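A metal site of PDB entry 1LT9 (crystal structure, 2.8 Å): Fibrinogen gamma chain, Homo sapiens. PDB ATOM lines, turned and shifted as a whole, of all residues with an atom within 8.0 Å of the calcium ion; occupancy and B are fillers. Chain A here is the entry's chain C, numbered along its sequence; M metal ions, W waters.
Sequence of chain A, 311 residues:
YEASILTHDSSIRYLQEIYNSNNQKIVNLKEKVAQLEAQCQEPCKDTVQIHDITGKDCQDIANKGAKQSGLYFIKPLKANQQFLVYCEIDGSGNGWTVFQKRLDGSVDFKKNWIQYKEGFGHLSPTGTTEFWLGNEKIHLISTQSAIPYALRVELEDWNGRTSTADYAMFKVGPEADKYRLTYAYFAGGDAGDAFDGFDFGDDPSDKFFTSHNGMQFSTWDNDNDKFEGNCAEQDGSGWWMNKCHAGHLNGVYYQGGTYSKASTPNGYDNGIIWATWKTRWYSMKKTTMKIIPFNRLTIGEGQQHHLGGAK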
ATOM      1  N   SER A 218     -21.272  15.150  16.394  1.00  0.00           N
ATOM      2  CA  SER A 218     -21.502  16.010  17.548  1.00  0.00           C
ATOM      3  C   SER A 218     -22.982  16.171  17.893  1.00  0.00           C
ATOM      4  O   SER A 218     -23.839  16.222  17.018  1.00  0.00           O
ATOM      5  CB  SER A 218     -20.901  17.413  17.316  1.00  0.00           C
ATOM      6  OG  SER A 218     -19.484  17.426  17.365  1.00  0.00           O
ATOM      7  N   ASN A 222     -22.414  16.598  23.777  1.00  0.00           N
ATOM      8  CA  ASN A 222     -21.119  15.996  23.453  1.00  0.00           C
ATOM      9  C   ASN A 222     -20.533  16.715  22.241  1.00  0.00           C
ATOM     10  O   ASN A 222     -20.704  16.278  21.108  1.00  0.00           O
ATOM     11  CB  ASN A 222     -21.296  14.496  23.181  1.00  0.00           C
ATOM     12  CG  ASN A 222     -19.975  13.729  23.249  1.00  0.00           C
ATOM     13  OD1 ASN A 222     -19.957  12.496  23.392  1.00  0.00           O
ATOM     14  ND2 ASN A 222     -18.857  14.452  23.125  1.00  0.00           N
ATOM     15  N   ASP A 223     -19.862  17.823  22.509  1.00  0.00           N
ATOM     16  CA  ASP A 223     -19.254  18.682  21.487  1.00  0.00           C
ATOM     17  C   ASP A 223     -17.936  18.098  20.979  1.00  0.00           C
ATOM     18  O   ASP A 223     -16.969  17.968  21.745  1.00  0.00           O
ATOM     19  CB  ASP A 223     -19.015  20.084  22.062  1.00  0.00           C
ATOM     20  CG  ASP A 223     -18.426  21.070  21.052  1.00  0.00           C
ATOM     21  OD1 ASP A 223     -17.429  20.738  20.368  1.00  0.00           O
ATOM     22  OD2 ASP A 223     -18.954  22.190  20.946  1.00  0.00           O
ATOM     23  N   ASN A 224     -17.900  17.762  19.702  1.00  0.00           N
ATOM     24  CA  ASN A 224     -16.697  17.208  19.096  1.00  0.00           C
ATOM     25  C   ASN A 224     -16.410  17.902  17.777  1.00  0.00           C
ATOM     26  O   ASN A 224     -15.842  17.309  16.859  1.00  0.00           O
ATOM     27  CB  ASN A 224     -16.873  15.696  18.869  1.00  0.00           C
ATOM     28  CG  ASN A 224     -16.926  14.912  20.167  1.00  0.00           C
ATOM     29  OD1 ASN A 224     -17.674  13.943  20.291  1.00  0.00           O
ATOM     30  ND2 ASN A 224     -16.116  15.309  21.140  1.00  0.00           N
ATOM     31  N   ASP A 225     -16.792  19.176  17.684  1.00  0.00           N
ATOM     32  CA  ASP A 225     -16.609  19.973  16.476  1.00  0.00           C
ATOM     33  C   ASP A 225     -15.297  20.775  16.456  1.00  0.00           C
ATOM     34  O   ASP A 225     -14.466  20.623  17.347  1.00  0.00           O
ATOM     35  CB  ASP A 225     -17.775  20.939  16.304  1.00  0.00           C
ATOM     36  CG  ASP A 225     -17.958  21.849  17.495  1.00  0.00           C
ATOM     37  OD1 ASP A 225     -16.954  22.131  18.173  1.00  0.00           O
ATOM     38  OD2 ASP A 225     -19.091  22.304  17.743  1.00  0.00           O
ATOM     39  N   LYS A 226     -15.135  21.608  15.431  1.00  0.00           N
ATOM     40  CA  LYS A 226     -13.947  22.442  15.251  1.00  0.00           C
ATOM     41  C   LYS A 226     -14.305  23.913  15.470  1.00  0.00           C
ATOM     42  O   LYS A 226     -13.813  24.799  14.762  1.00  0.00           O
ATOM     43  CB  LYS A 226     -13.375  22.274  13.848  1.00  0.00           C
ATOM     44  CG  LYS A 226     -12.940  20.865  13.504  1.00  0.00           C
ATOM     45  CD  LYS A 226     -11.762  20.423  14.358  1.00  0.00           C
ATOM     46  CE  LYS A 226     -11.307  19.018  13.972  1.00  0.00           C
ATOM     47  NZ  LYS A 226     -10.126  18.605  14.776  1.00  0.00           N
ATOM     48  N   PHE A 227     -15.165  24.167  16.444  1.00  0.00           N
ATOM     49  CA  PHE A 227     -15.620  25.509  16.778  1.00  0.00           C
ATOM     50  C   PHE A 227     -15.524  25.757  18.280  1.00  0.00           C
ATOM     51  O   PHE A 227     -15.705  24.849  19.084  1.00  0.00           O
ATOM     52  CB  PHE A 227     -17.061  25.681  16.299  1.00  0.00           C
ATOM     53  CG  PHE A 227     -17.668  27.014  16.654  1.00  0.00           C
ATOM     54  CD1 PHE A 227     -16.956  28.184  16.508  1.00  0.00           C
ATOM     55  CD2 PHE A 227     -18.988  27.077  17.101  1.00  0.00           C
ATOM     56  CE1 PHE A 227     -17.535  29.412  16.807  1.00  0.00           C
ATOM     57  CE2 PHE A 227     -19.577  28.294  17.400  1.00  0.00           C
ATOM     58  CZ  PHE A 227     -18.857  29.468  17.248  1.00  0.00           C
ATOM     59  N   GLU A 228     -15.211  26.994  18.652  1.00  0.00           N
ATOM     60  CA  GLU A 228     -15.095  27.370  20.060  1.00  0.00           C
ATOM     61  C   GLU A 228     -16.406  27.101  20.785  1.00  0.00           C
ATOM     62  O   GLU A 228     -16.410  26.723  21.953  1.00  0.00           O
ATOM     63  CB  GLU A 228     -14.720  28.856  20.184  1.00  0.00           C
ATOM     64  CG  GLU A 228     -14.783  29.425  21.603  1.00  0.00           C
ATOM     65  CD  GLU A 228     -13.799  28.762  22.567  1.00  0.00           C
ATOM     66  OE1 GLU A 228     -13.717  29.218  23.733  1.00  0.00           O
ATOM     67  OE2 GLU A 228     -13.119  27.790  22.158  1.00  0.00           O
ATOM     68  N   GLY A 229     -17.508  27.300  20.071  1.00  0.00           N
ATOM     69  CA  GLY A 229     -18.820  27.068  20.643  1.00  0.00           C
ATOM     70  C   GLY A 229     -19.331  25.671  20.357  1.00  0.00           C
ATOM     71  O   GLY A 229     -18.562  24.745  20.105  1.00  0.00           O
ATOM     72  N   ASN A 230     -20.654  25.525  20.392  1.00  0.00           N
ATOM     73  CA  ASN A 230     -21.259  24.225  20.175  1.00  0.00           C
ATOM     74  C   ASN A 230     -22.191  24.200  18.971  1.00  0.00           C
ATOM     75  O   ASN A 230     -23.346  24.616  19.083  1.00  0.00           O
ATOM     76  CB  ASN A 230     -22.018  23.832  21.427  1.00  0.00           C
ATOM     77  CG  ASN A 230     -22.492  22.409  21.398  1.00  0.00           C
ATOM     78  OD1 ASN A 230     -22.976  21.904  22.393  1.00  0.00           O
ATOM     79  ND2 ASN A 230     -22.345  21.751  20.264  1.00  0.00           N
ATOM     80  N   CYS A 231     -21.695  23.707  17.845  1.00  0.00           N
ATOM     81  CA  CYS A 231     -22.511  23.648  16.634  1.00  0.00           C
ATOM     82  C   CYS A 231     -23.820  22.915  16.885  1.00  0.00           C
ATOM     83  O   CYS A 231     -24.897  23.475  16.710  1.00  0.00           O
ATOM     84  CB  CYS A 231     -21.752  22.946  15.509  1.00  0.00           C
ATOM     85  SG  CYS A 231     -20.305  23.860  14.897  1.00  0.00           S
ATOM     86  N   ALA A 232     -23.695  21.642  17.283  1.00  0.00           N
ATOM     87  CA  ALA A 232     -24.843  20.796  17.559  1.00  0.00           C
ATOM     88  C   ALA A 232     -25.886  21.524  18.418  1.00  0.00           C
ATOM     89  O   ALA A 232     -27.084  21.436  18.146  1.00  0.00           O
ATOM     90  CB  ALA A 232     -24.392  19.531  18.264  1.00  0.00           C
ATOM     91  N   MET A 241     -20.354  18.009  12.761  1.00  0.00           N
ATOM     92  CA  MET A 241     -20.078  19.428  12.756  1.00  0.00           C
ATOM     93  C   MET A 241     -18.605  19.765  12.674  1.00  0.00           C
ATOM     94  O   MET A 241     -17.750  19.068  13.227  1.00  0.00           O
ATOM     95  CB  MET A 241     -20.668  20.070  14.014  1.00  0.00           C
ATOM     96  CG  MET A 241     -22.178  19.940  14.144  1.00  0.00           C
ATOM     97  SD  MET A 241     -23.106  20.734  12.807  1.00  0.00           S
ATOM     98  CE  MET A 241     -24.766  20.687  13.477  1.00  0.00           C
ATOM     99  N   ASN A 242     -18.334  20.853  11.962  1.00  0.00           N
ATOM    100  CA  ASN A 242     -16.998  21.371  11.784  1.00  0.00           C
ATOM    101  C   ASN A 242     -16.989  22.752  12.447  1.00  0.00           C
ATOM    102  O   ASN A 242     -16.592  22.898  13.593  1.00  0.00           O
ATOM    103  CB  ASN A 242     -16.687  21.482  10.281  1.00  0.00           C
ATOM    104  CG  ASN A 242     -15.300  22.035  10.000  1.00  0.00           C
ATOM    105  OD1 ASN A 242     -14.947  22.232   8.839  1.00  0.00           O
ATOM    106  ND2 ASN A 242     -14.522  22.278  11.037  1.00  0.00           N
ATOM    107  N   CYS A 244     -19.502  25.694  10.885  1.00  0.00           N
ATOM    108  CA  CYS A 244     -20.122  24.463  11.359  1.00  0.00           C
ATOM    109  C   CYS A 244     -20.510  23.482  10.252  1.00  0.00           C
ATOM    110  O   CYS A 244     -20.205  22.294  10.343  1.00  0.00           O
ATOM    111  CB  CYS A 244     -21.368  24.770  12.189  1.00  0.00           C
ATOM    112  SG  CYS A 244     -21.115  25.415  13.870  1.00  0.00           S
HETATM  113 CA    CA M   1     -16.826  23.206  20.168  1.00  0.00          CA
HETATM  114  O   HOH W   1     -14.941  21.828  19.873  1.00  0.00           O
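Glu 228 touches the calcium ion. Of the 15 residues printed, 5 come within 4 Å of the calcium ion.
SG of Cys 231 forms a disulfide with SG of Cys 244 (2.0 Å). The side-chain carboxylate (OD2) of Asp 225 sits at hydrogen-bond distance from the backbone NH (N) of Cys 231, at 3.0 Å. N of Asp 225 lies within hydrogen-bond range of OG of Ser 218. ND2 of Asn 230 lies close to OD2 of Asp 223 (3.5 Å). The backbone NH of Phe 227 lies within hydrogen-bond range of the backbone carbonyl oxygen of Asn 242 (3.4 Å).
The backbone carbonyl oxygen (O) of Phe 227 is bound to the calcium ion, 2.3 Å away. OD1 of Asp 225 is bound to the calcium ion, at 2.3 Å. The backbone carbonyl oxygen (O) of Gly 229 binds the calcium ion (2.3 Å). The calcium ion is bound by water W1 (2.4 Å). The calcium ion is bound by OD2 of Asp 223 (2.5 Å). OD1 of Asp 223 binds the calcium ion.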
